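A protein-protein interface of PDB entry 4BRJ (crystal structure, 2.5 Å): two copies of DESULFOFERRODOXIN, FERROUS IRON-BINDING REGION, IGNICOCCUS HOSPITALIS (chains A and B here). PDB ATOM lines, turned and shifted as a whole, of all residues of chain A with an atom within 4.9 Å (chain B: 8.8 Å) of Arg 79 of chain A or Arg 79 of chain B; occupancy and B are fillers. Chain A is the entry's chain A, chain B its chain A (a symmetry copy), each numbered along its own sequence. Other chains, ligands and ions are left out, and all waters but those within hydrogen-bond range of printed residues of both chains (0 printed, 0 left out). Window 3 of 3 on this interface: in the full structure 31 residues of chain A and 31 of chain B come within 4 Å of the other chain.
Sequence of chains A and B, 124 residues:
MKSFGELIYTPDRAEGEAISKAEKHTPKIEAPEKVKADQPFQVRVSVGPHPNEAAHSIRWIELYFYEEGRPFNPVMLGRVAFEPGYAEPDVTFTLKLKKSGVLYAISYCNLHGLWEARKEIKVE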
ATOM      1  N   TRP A  60      21.415   1.025  -1.187  1.00  0.00           N
ATOM      2  CA  TRP A  60      20.462  -0.003  -1.617  1.00  0.00           C
ATOM      3  C   TRP A  60      20.914  -0.858  -2.808  1.00  0.00           C
ATOM      4  O   TRP A  60      21.758  -0.449  -3.605  1.00  0.00           O
ATOM      5  CB  TRP A  60      19.087   0.622  -1.916  1.00  0.00           C
ATOM      6  CG  TRP A  60      19.103   1.826  -2.877  1.00  0.00           C
ATOM      7  CD1 TRP A  60      18.994   3.138  -2.530  1.00  0.00           C
ATOM      8  CD2 TRP A  60      19.217   1.806  -4.321  1.00  0.00           C
ATOM      9  NE1 TRP A  60      19.024   3.934  -3.646  1.00  0.00           N
ATOM     10  CE2 TRP A  60      19.156   3.147  -4.761  1.00  0.00           C
ATOM     11  CE3 TRP A  60      19.346   0.788  -5.278  1.00  0.00           C
ATOM     12  CZ2 TRP A  60      19.251   3.508  -6.125  1.00  0.00           C
ATOM     13  CZ3 TRP A  60      19.430   1.149  -6.647  1.00  0.00           C
ATOM     14  CH2 TRP A  60      19.378   2.499  -7.046  1.00  0.00           C
ATOM     15  N   ILE A  61      20.328  -2.045  -2.922  1.00  0.00           N
ATOM     16  CA  ILE A  61      20.557  -2.892  -4.079  1.00  0.00           C
ATOM     17  C   ILE A  61      19.256  -3.224  -4.819  1.00  0.00           C
ATOM     18  O   ILE A  61      18.256  -3.601  -4.205  1.00  0.00           O
ATOM     19  CB  ILE A  61      21.346  -4.163  -3.705  1.00  0.00           C
ATOM     20  CG1 ILE A  61      22.810  -3.799  -3.412  1.00  0.00           C
ATOM     21  CG2 ILE A  61      21.301  -5.163  -4.843  1.00  0.00           C
ATOM     22  CD1 ILE A  61      23.627  -4.955  -2.852  1.00  0.00           C
ATOM     23  N   GLU A  62      19.262  -3.048  -6.140  1.00  0.00           N
ATOM     24  CA  GLU A  62      18.111  -3.441  -6.970  1.00  0.00           C
ATOM     25  C   GLU A  62      18.455  -4.665  -7.803  1.00  0.00           C
ATOM     26  O   GLU A  62      19.544  -4.742  -8.383  1.00  0.00           O
ATOM     27  CB  GLU A  62      17.629  -2.299  -7.872  1.00  0.00           C
ATOM     28  CG  GLU A  62      16.784  -1.248  -7.160  1.00  0.00           C
ATOM     29  CD  GLU A  62      16.441  -0.051  -8.052  1.00  0.00           C
ATOM     30  OE1 GLU A  62      17.077   0.110  -9.119  1.00  0.00           O
ATOM     31  OE2 GLU A  62      15.541   0.734  -7.680  1.00  0.00           O
ATOM     32  N   MET A  76      11.674  -6.002 -12.719  1.00  0.00           N
ATOM     33  CA  MET A  76      12.317  -5.840 -11.414  1.00  0.00           C
ATOM     34  C   MET A  76      11.908  -6.964 -10.469  1.00  0.00           C
ATOM     35  O   MET A  76      10.728  -7.184 -10.260  1.00  0.00           O
ATOM     36  CB  MET A  76      11.970  -4.501 -10.772  1.00  0.00           C
ATOM     37  CG  MET A  76      12.654  -4.341  -9.427  1.00  0.00           C
ATOM     38  SD  MET A  76      12.129  -2.888  -8.525  1.00  0.00           S
ATOM     39  CE  MET A  76      13.690  -2.012  -8.442  1.00  0.00           C
ATOM     40  N   LEU A  77      12.890  -7.648  -9.894  1.00  0.00           N
ATOM     41  CA  LEU A  77      12.666  -8.828  -9.057  1.00  0.00           C
ATOM     42  C   LEU A  77      12.553  -8.496  -7.565  1.00  0.00           C
ATOM     43  O   LEU A  77      11.728  -9.074  -6.838  1.00  0.00           O
ATOM     44  CB  LEU A  77      13.812  -9.831  -9.261  1.00  0.00           C
ATOM     45  CG  LEU A  77      13.910 -10.448 -10.665  1.00  0.00           C
ATOM     46  CD1 LEU A  77      14.922 -11.606 -10.724  1.00  0.00           C
ATOM     47  CD2 LEU A  77      12.503 -10.875 -11.156  1.00  0.00           C
ATOM     48  N   GLY A  78      13.401  -7.571  -7.117  1.00  0.00           N
ATOM     49  CA  GLY A  78      13.456  -7.183  -5.728  1.00  0.00           C
ATOM     50  C   GLY A  78      14.224  -5.899  -5.490  1.00  0.00           C
ATOM     51  O   GLY A  78      14.939  -5.414  -6.353  1.00  0.00           O
ATOM     52  N   ARG A  79      14.045  -5.328  -4.309  1.00  0.00           N
ATOM     53  CA  ARG A  79      14.802  -4.158  -3.910  1.00  0.00           C
ATOM     54  C   ARG A  79      15.049  -4.244  -2.419  1.00  0.00           C
ATOM     55  O   ARG A  79      14.144  -4.500  -1.643  1.00  0.00           O
ATOM     56  CB  ARG A  79      14.072  -2.861  -4.277  1.00  0.00           C
ATOM     57  CG  ARG A  79      14.882  -1.614  -3.992  1.00  0.00           C
ATOM     58  CD  ARG A  79      14.282  -0.341  -4.586  1.00  0.00           C
ATOM     59  NE  ARG A  79      14.489   0.771  -3.656  1.00  0.00           N
ATOM     60  CZ  ARG A  79      15.327   1.777  -3.859  1.00  0.00           C
ATOM     61  NH1 ARG A  79      16.029   1.843  -4.985  1.00  0.00           N
ATOM     62  NH2 ARG A  79      15.445   2.729  -2.948  1.00  0.00           N
ATOM     63  N   VAL A  80      16.292  -4.060  -2.016  1.00  0.00           N
ATOM     64  CA  VAL A  80      16.588  -4.051  -0.609  1.00  0.00           C
ATOM     65  C   VAL A  80      17.312  -2.758  -0.237  1.00  0.00           C
ATOM     66  O   VAL A  80      18.178  -2.290  -0.975  1.00  0.00           O
ATOM     67  CB  VAL A  80      17.418  -5.275  -0.206  1.00  0.00           C
ATOM     68  CG1 VAL A  80      18.684  -5.375  -1.074  1.00  0.00           C
ATOM     69  CG2 VAL A  80      17.746  -5.215   1.313  1.00  0.00           C
ATOM     70  N   ALA A  81      16.937  -2.178   0.904  1.00  0.00           N
ATOM     71  CA  ALA A  81      17.611  -0.986   1.406  1.00  0.00           C
ATOM     72  C   ALA A  81      18.283  -1.324   2.724  1.00  0.00           C
ATOM     73  O   ALA A  81      17.718  -2.069   3.540  1.00  0.00           O
ATOM     74  CB  ALA A  81      16.636   0.158   1.578  1.00  0.00           C
ATOM     75  N   PHE A  93      18.210 -13.522  -1.866  1.00  0.00           N
ATOM     76  CA  PHE A  93      16.827 -13.622  -2.310  1.00  0.00           C
ATOM     77  C   PHE A  93      16.488 -15.057  -2.636  1.00  0.00           C
ATOM     78  O   PHE A  93      17.376 -15.867  -2.892  1.00  0.00           O
ATOM     79  CB  PHE A  93      16.617 -12.816  -3.582  1.00  0.00           C
ATOM     80  CG  PHE A  93      16.550 -11.332  -3.372  1.00  0.00           C
ATOM     81  CD1 PHE A  93      15.333 -10.710  -3.141  1.00  0.00           C
ATOM     82  CD2 PHE A  93      17.696 -10.553  -3.456  1.00  0.00           C
ATOM     83  CE1 PHE A  93      15.255  -9.331  -2.977  1.00  0.00           C
ATOM     84  CE2 PHE A  93      17.635  -9.183  -3.294  1.00  0.00           C
ATOM     85  CZ  PHE A  93      16.416  -8.563  -3.056  1.00  0.00           C
ATOM     86  N   ARG B  59       4.194   1.180 -11.076  1.00  0.00           N
ATOM     87  CA  ARG B  59       4.524   0.815  -9.704  1.00  0.00           C
ATOM     88  C   ARG B  59       5.252   1.929  -8.950  1.00  0.00           C
ATOM     89  O   ARG B  59       4.892   2.242  -7.825  1.00  0.00           O
ATOM     90  CB  ARG B  59       5.360  -0.466  -9.641  1.00  0.00           C
ATOM     91  CG  ARG B  59       4.752  -1.669 -10.354  1.00  0.00           C
ATOM     92  CD  ARG B  59       3.332  -2.028  -9.890  1.00  0.00           C
ATOM     93  NE  ARG B  59       3.098  -3.468 -10.035  1.00  0.00           N
ATOM     94  CZ  ARG B  59       1.937  -4.030 -10.388  1.00  0.00           C
ATOM     95  NH1 ARG B  59       0.867  -3.284 -10.660  1.00  0.00           N
ATOM     96  NH2 ARG B  59       1.850  -5.355 -10.484  1.00  0.00           N
ATOM     97  N   TRP B  60       6.269   2.532  -9.564  1.00  0.00           N
ATOM     98  CA  TRP B  60       7.063   3.537  -8.849  1.00  0.00           C
ATOM     99  C   TRP B  60       7.779   4.560  -9.739  1.00  0.00           C
ATOM    100  O   TRP B  60       8.043   4.311 -10.915  1.00  0.00           O
ATOM    101  CB  TRP B  60       8.080   2.860  -7.911  1.00  0.00           C
ATOM    102  CG  TRP B  60       8.970   1.786  -8.566  1.00  0.00           C
ATOM    103  CD1 TRP B  60       8.823   0.438  -8.455  1.00  0.00           C
ATOM    104  CD2 TRP B  60      10.136   1.991  -9.401  1.00  0.00           C
ATOM    105  NE1 TRP B  60       9.810  -0.211  -9.151  1.00  0.00           N
ATOM    106  CE2 TRP B  60      10.633   0.713  -9.740  1.00  0.00           C
ATOM    107  CE3 TRP B  60      10.812   3.125  -9.878  1.00  0.00           C
ATOM    108  CZ2 TRP B  60      11.766   0.528 -10.565  1.00  0.00           C
ATOM    109  CZ3 TRP B  60      11.955   2.941 -10.696  1.00  0.00           C
ATOM    110  CH2 TRP B  60      12.413   1.648 -11.023  1.00  0.00           C
ATOM    111  N   ILE B  61       8.101   5.709  -9.156  1.00  0.00           N
ATOM    112  CA  ILE B  61       8.906   6.705  -9.841  1.00  0.00           C
ATOM    113  C   ILE B  61      10.194   7.035  -9.075  1.00  0.00           C
ATOM    114  O   ILE B  61      10.169   7.264  -7.865  1.00  0.00           O
ATOM    115  CB  ILE B  61       8.088   7.972 -10.163  1.00  0.00           C
ATOM    116  CG1 ILE B  61       7.099   7.676 -11.300  1.00  0.00           C
ATOM    117  CG2 ILE B  61       9.010   9.097 -10.587  1.00  0.00           C
ATOM    118  CD1 ILE B  61       6.116   8.808 -11.565  1.00  0.00           C
ATOM    119  N   GLU B  62      11.324   7.023  -9.780  1.00  0.00           N
ATOM    120  CA  GLU B  62      12.604   7.434  -9.181  1.00  0.00           C
ATOM    121  C   GLU B  62      13.048   8.772  -9.751  1.00  0.00           C
ATOM    122  O   GLU B  62      12.965   8.993 -10.965  1.00  0.00           O
ATOM    123  CB  GLU B  62      13.700   6.381  -9.374  1.00  0.00           C
ATOM    124  CG  GLU B  62      13.610   5.195  -8.420  1.00  0.00           C
ATOM    125  CD  GLU B  62      14.630   4.096  -8.733  1.00  0.00           C
ATOM    126  OE1 GLU B  62      15.215   4.110  -9.841  1.00  0.00           O
ATOM    127  OE2 GLU B  62      14.839   3.211  -7.874  1.00  0.00           O
ATOM    128  N   LEU B  63      13.486   9.668  -8.868  1.00  0.00           N
ATOM    129  CA  LEU B  63      13.976  10.986  -9.275  1.00  0.00           C
ATOM    130  C   LEU B  63      15.443  11.076  -8.943  1.00  0.00           C
ATOM    131  O   LEU B  63      15.823  10.963  -7.779  1.00  0.00           O
ATOM    132  CB  LEU B  63      13.220  12.113  -8.573  1.00  0.00           C
ATOM    133  CG  LEU B  63      13.530  13.560  -8.972  1.00  0.00           C
ATOM    134  CD1 LEU B  63      13.265  13.815 -10.456  1.00  0.00           C
ATOM    135  CD2 LEU B  63      12.739  14.565  -8.120  1.00  0.00           C
ATOM    136  N   TYR B  64      16.260  11.249  -9.986  1.00  0.00           N
ATOM    137  CA  TYR B  64      17.704  11.360  -9.855  1.00  0.00           C
ATOM    138  C   TYR B  64      18.169  12.729 -10.360  1.00  0.00           C
ATOM    139  O   TYR B  64      17.393  13.473 -10.969  1.00  0.00           O
ATOM    140  CB  TYR B  64      18.399  10.296 -10.696  1.00  0.00           C
ATOM    141  CG  TYR B  64      18.311   8.860 -10.232  1.00  0.00           C
ATOM    142  CD1 TYR B  64      19.282   8.326  -9.397  1.00  0.00           C
ATOM    143  CD2 TYR B  64      17.289   8.020 -10.680  1.00  0.00           C
ATOM    144  CE1 TYR B  64      19.242   7.000  -8.988  1.00  0.00           C
ATOM    145  CE2 TYR B  64      17.224   6.684 -10.275  1.00  0.00           C
ATOM    146  CZ  TYR B  64      18.206   6.175  -9.422  1.00  0.00           C
ATOM    147  OH  TYR B  64      18.161   4.847  -9.016  1.00  0.00           O
ATOM    148  N   MET B  76      20.681  10.231  -6.355  1.00  0.00           N
ATOM    149  CA  MET B  76      19.247   9.956  -6.250  1.00  0.00           C
ATOM    150  C   MET B  76      18.582  10.924  -5.279  1.00  0.00           C
ATOM    151  O   MET B  76      19.006  11.036  -4.144  1.00  0.00           O
ATOM    152  CB  MET B  76      18.975   8.527  -5.789  1.00  0.00           C
ATOM    153  CG  MET B  76      17.486   8.251  -5.698  1.00  0.00           C
ATOM    154  SD  MET B  76      17.094   6.667  -4.967  1.00  0.00           S
ATOM    155  CE  MET B  76      16.267   5.896  -6.358  1.00  0.00           C
ATOM    156  N   LEU B  77      17.532  11.599  -5.735  1.00  0.00           N
ATOM    157  CA  LEU B  77      16.857  12.650  -4.970  1.00  0.00           C
ATOM    158  C   LEU B  77      15.673  12.131  -4.149  1.00  0.00           C
ATOM    159  O   LEU B  77      15.447  12.557  -3.004  1.00  0.00           O
ATOM    160  CB  LEU B  77      16.362  13.746  -5.925  1.00  0.00           C
ATOM    161  CG  LEU B  77      17.460  14.536  -6.655  1.00  0.00           C
ATOM    162  CD1 LEU B  77      16.902  15.759  -7.403  1.00  0.00           C
ATOM    163  CD2 LEU B  77      18.585  14.922  -5.659  1.00  0.00           C
ATOM    164  N   GLY B  78      14.912  11.219  -4.751  1.00  0.00           N
ATOM    165  CA  GLY B  78      13.729  10.668  -4.133  1.00  0.00           C
ATOM    166  C   GLY B  78      13.214   9.420  -4.819  1.00  0.00           C
ATOM    167  O   GLY B  78      13.605   9.095  -5.929  1.00  0.00           O
ATOM    168  N   ARG B  79      12.343   8.698  -4.130  1.00  0.00           N
ATOM    169  CA  ARG B  79      11.689   7.543  -4.711  1.00  0.00           C
ATOM    170  C   ARG B  79      10.287   7.463  -4.145  1.00  0.00           C
ATOM    171  O   ARG B  79      10.085   7.560  -2.946  1.00  0.00           O
ATOM    172  CB  ARG B  79      12.471   6.254  -4.439  1.00  0.00           C
ATOM    173  CG  ARG B  79      11.891   5.040  -5.133  1.00  0.00           C
ATOM    174  CD  ARG B  79      12.797   3.810  -5.084  1.00  0.00           C
ATOM    175  NE  ARG B  79      11.975   2.610  -4.919  1.00  0.00           N
ATOM    176  CZ  ARG B  79      11.778   1.696  -5.857  1.00  0.00           C
ATOM    177  NH1 ARG B  79      12.371   1.817  -7.040  1.00  0.00           N
ATOM    178  NH2 ARG B  79      11.008   0.650  -5.606  1.00  0.00           N
ATOM    179  N   VAL B  80       9.307   7.317  -5.016  1.00  0.00           N
ATOM    180  CA  VAL B  80       7.958   7.156  -4.546  1.00  0.00           C
ATOM    181  C   VAL B  80       7.351   5.880  -5.128  1.00  0.00           C
ATOM    182  O   VAL B  80       7.557   5.566  -6.301  1.00  0.00           O
ATOM    183  CB  VAL B  80       7.097   8.376  -4.893  1.00  0.00           C
ATOM    184  CG1 VAL B  80       7.165   8.668  -6.403  1.00  0.00           C
ATOM    185  CG2 VAL B  80       5.640   8.153  -4.400  1.00  0.00           C
ATOM    186  N   ALA B  81       6.618   5.140  -4.294  1.00  0.00           N
ATOM    187  CA  ALA B  81       5.921   3.945  -4.755  1.00  0.00           C
ATOM    188  C   ALA B  81       4.427   4.165  -4.606  1.00  0.00           C
ATOM    189  O   ALA B  81       3.979   4.764  -3.617  1.00  0.00           O
ATOM    190  CB  ALA B  81       6.364   2.724  -3.978  1.00  0.00           C
ATOM    191  N   PHE B  82       3.669   3.705  -5.604  1.00  0.00           N
ATOM    192  CA  PHE B  82       2.217   3.885  -5.639  1.00  0.00           C
ATOM    193  C   PHE B  82       1.503   2.545  -5.513  1.00  0.00           C
ATOM    194  O   PHE B  82       1.891   1.565  -6.156  1.00  0.00           O
ATOM    195  CB  PHE B  82       1.770   4.552  -6.946  1.00  0.00           C
ATOM    196  CG  PHE B  82       2.577   5.768  -7.329  1.00  0.00           C
ATOM    197  CD1 PHE B  82       2.465   6.955  -6.614  1.00  0.00           C
ATOM    198  CD2 PHE B  82       3.432   5.732  -8.434  1.00  0.00           C
ATOM    199  CE1 PHE B  82       3.210   8.081  -6.974  1.00  0.00           C
ATOM    200  CE2 PHE B  82       4.172   6.854  -8.810  1.00  0.00           C
ATOM    201  CZ  PHE B  82       4.056   8.031  -8.087  1.00  0.00           C
ATOM    202  N   VAL B  91       3.216  12.842  -8.513  1.00  0.00           N
ATOM    203  CA  VAL B  91       3.871  13.167  -7.259  1.00  0.00           C
ATOM    204  C   VAL B  91       4.571  14.516  -7.323  1.00  0.00           C
ATOM    205  O   VAL B  91       5.108  14.903  -8.358  1.00  0.00           O
ATOM    206  CB  VAL B  91       4.885  12.070  -6.866  1.00  0.00           C
ATOM    207  CG1 VAL B  91       5.930  11.885  -7.959  1.00  0.00           C
ATOM    208  CG2 VAL B  91       5.551  12.382  -5.498  1.00  0.00           C
ATOM    209  N   PHE B  93       7.527  16.798  -5.411  1.00  0.00           N
ATOM    210  CA  PHE B  93       8.620  16.857  -4.452  1.00  0.00           C
ATOM    211  C   PHE B  93       8.977  18.294  -4.156  1.00  0.00           C
ATOM    212  O   PHE B  93       8.673  19.188  -4.943  1.00  0.00           O
ATOM    213  CB  PHE B  93       9.866  16.200  -5.026  1.00  0.00           C
ATOM    214  CG  PHE B  93       9.824  14.701  -5.043  1.00  0.00           C
ATOM    215  CD1 PHE B  93      10.308  13.972  -3.967  1.00  0.00           C
ATOM    216  CD2 PHE B  93       9.349  14.017  -6.154  1.00  0.00           C
ATOM    217  CE1 PHE B  93      10.304  12.582  -3.984  1.00  0.00           C
ATOM    218  CE2 PHE B  93       9.338  12.638  -6.187  1.00  0.00           C
ATOM    219  CZ  PHE B  93       9.817  11.911  -5.106  1.00  0.00           C
ATOM    220  N   ILE B 106      12.562   8.284 -13.623  1.00  0.00           N
ATOM    221  CA  ILE B 106      12.373   6.916 -14.081  1.00  0.00           C
ATOM    222  C   ILE B 106      11.053   6.296 -13.577  1.00  0.00           C
ATOM    223  O   ILE B 106      10.825   6.150 -12.364  1.00  0.00           O
ATOM    224  CB  ILE B 106      13.559   6.023 -13.719  1.00  0.00           C
ATOM    225  CG1 ILE B 106      14.881   6.690 -14.128  1.00  0.00           C
ATOM    226  CG2 ILE B 106      13.398   4.681 -14.401  1.00  0.00           C
ATOM    227  CD1 ILE B 106      15.016   6.923 -15.638  1.00  0.00           C
ATOM    228  N   SER B 107      10.178   5.956 -14.517  1.00  0.00           N
ATOM    229  CA  SER B 107       8.928   5.274 -14.184  1.00  0.00           C
ATOM    230  C   SER B 107       9.075   3.785 -14.444  1.00  0.00           C
ATOM    231  O   SER B 107       9.770   3.372 -15.385  1.00  0.00           O
ATOM    232  CB  SER B 107       7.761   5.829 -14.992  1.00  0.00           C
ATOM    233  OG  SER B 107       7.994   5.599 -16.371  1.00  0.00           O
ATOM    234  N   TYR B 108       8.431   2.978 -13.598  1.00  0.00           N
ATOM    235  CA  TYR B 108       8.418   1.531 -13.804  1.00  0.00           C
ATOM    236  C   TYR B 108       6.996   1.007 -13.966  1.00  0.00           C
ATOM    237  O   TYR B 108       6.130   1.281 -13.147  1.00  0.00           O
ATOM    238  CB  TYR B 108       9.176   0.778 -12.700  1.00  0.00           C
ATOM    239  CG  TYR B 108       9.135  -0.726 -12.873  1.00  0.00           C
ATOM    240  CD1 TYR B 108       9.861  -1.339 -13.898  1.00  0.00           C
ATOM    241  CD2 TYR B 108       8.354  -1.535 -12.036  1.00  0.00           C
ATOM    242  CE1 TYR B 108       9.825  -2.722 -14.090  1.00  0.00           C
ATOM    243  CE2 TYR B 108       8.312  -2.924 -12.210  1.00  0.00           C
ATOM    244  CZ  TYR B 108       9.053  -3.512 -13.253  1.00  0.00           C
ATOM    245  OH  TYR B 108       9.046  -4.876 -13.476  1.00  0.00           O
ATOM    246  N   LEU B 114      11.054   0.130 -17.930  1.00  0.00           N
ATOM    247  CA  LEU B 114      11.630   1.378 -17.405  1.00  0.00           C
ATOM    248  C   LEU B 114      11.656   2.504 -18.425  1.00  0.00           C
ATOM    249  O   LEU B 114      12.243   2.371 -19.515  1.00  0.00           O
ATOM    250  CB  LEU B 114      13.047   1.129 -16.886  1.00  0.00           C
ATOM    251  CG  LEU B 114      13.192   0.149 -15.716  1.00  0.00           C
ATOM    252  CD1 LEU B 114      14.642  -0.353 -15.581  1.00  0.00           C
ATOM    253  CD2 LEU B 114      12.686   0.790 -14.415  1.00  0.00           C
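The side-chain sulfur (SD) of Met 76 of chain B sits at hydrogen-bond distance from the indole nitrogen (NE1) of Trp 60 of chain A.
The side-chain carboxylate of Glu 62 of chain A sits close to the side-chain carboxylate of Glu 62 of chain B (2.6 Å).
OE2 of Glu 62 of chain A lies within salt-bridge range of NH1 of Arg 79 of chain B (3.4 Å).
The side-chain sulfur (SD) of Met 76 of chain A is in hydrogen-bond range of the indole nitrogen (NE1) of Trp 60 of chain B (3.6 Å).
The side-chain hydroxyl (OH) of Tyr 108 of chain B sits at hydrogen-bond distance from the backbone NH (N) of Met 76 of chain A.
NH1 of Arg 79 of chain A lies within salt-bridge range of OE2 of Glu 62 of chain B, at 3.4 Å.
The guanidinium group (NE) of Arg 79 of chain A lies close to the guanidinium group (NE) of Arg 79 of chain B (3.4 Å).
Trp 60 of chain A touches Met 76 of chain B, and with the chains exchanged Met 76 of chain A touches Trp 60 of chain B.
Glu 62 of chain B touches its own counterpart, Glu 62 of chain A.
Glu 62 of chain A touches Arg 79 of chain B, and with the chains exchanged Arg 79 of chain A touches Glu 62 of chain B.
Arg 79 of chain A touches its own counterpart, Arg 79 of chain B.
Positions printed for both chains: 60, 61, 62, 76, 77, 78, 79, 80, 81 and 93.
Of the 8 pairs that touch across the chains among the printed residues, 6 have their exchanged pair printed and touching as well.
The guanidinium group (NH1) of Arg 79 of chain A is in salt-bridge range of the side-chain carboxylate (OE2) of Glu 62 of chain A.
The backbone NH (N) of Arg 59 of chain B is in hydrogen-bond range of the backbone carbonyl oxygen (O) of Tyr 108 of chain B (2.8 Å).
The backbone carbonyl oxygen (O) of Trp 60 of chain B lies within hydrogen-bond range of the backbone NH (N) of Tyr 108 of chain B.
The side-chain carboxylate (OE1) of Glu 62 of chain B lies within hydrogen-bond range of the side-chain hydroxyl (OH) of Tyr 64 of chain B (3.1 Å).
The side-chain carboxylate (OE2) of Glu 62 of chain B lies within salt-bridge range of the guanidinium group (NH1) of Arg 79 of chain B (3.0 Å).
N of Glu 62 of chain B sits at hydrogen-bond distance from O of Ile 106 of chain B.
Of chain B, only Glu 62 and Arg 79 come within 4 Å of Arg 79 of chain A.
Of chain A, only Glu 62 (3.4 Å) and Arg 79 (3.4 Å) come within 4 Å of Arg 79 of chain B.
Gly 78 of chain A touches none of the printed residues of chain B.
Of the printed residues of chain A, Tyr 108 of chain B touches Met 76.
Printed residues of chain A within 4 Å of Trp 60 of chain B: Met 76.
Printed residues of chain B within 4 Å of Met 76 of chain A: Trp 60 (3.6 Å) and Tyr 108 (3.0 Å).
Of the printed residues of chain B, Trp 60 of chain A touches Tyr 64 (3.3 Å) and Met 76 (3.6 Å).
Of the printed residues of chain B, Glu 62 of chain A touches Glu 62 (2.6 Å) and Arg 79 (3.4 Å).
Ser 107 of chain B touches none of the printed residues of chain A.
The nearest printed residue of chain B that does not touch Glu 62 of chain A is Trp 60 of chain B (4.7 Å).
Of the 19 printed residues of chain B, 6 touch a printed residue of chain A.
Printed residues of chain A that touch a printed residue of chain B: Trp 60, Glu 62, Met 76 and Arg 79.
Hydrophobic or aromatic side chains of chain A that line the printed part of chain B: Trp 60 and Met 76.
Tyr 64 of chain B touches Trp 60 of chain A (OH to CH2, 3.3 Å).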
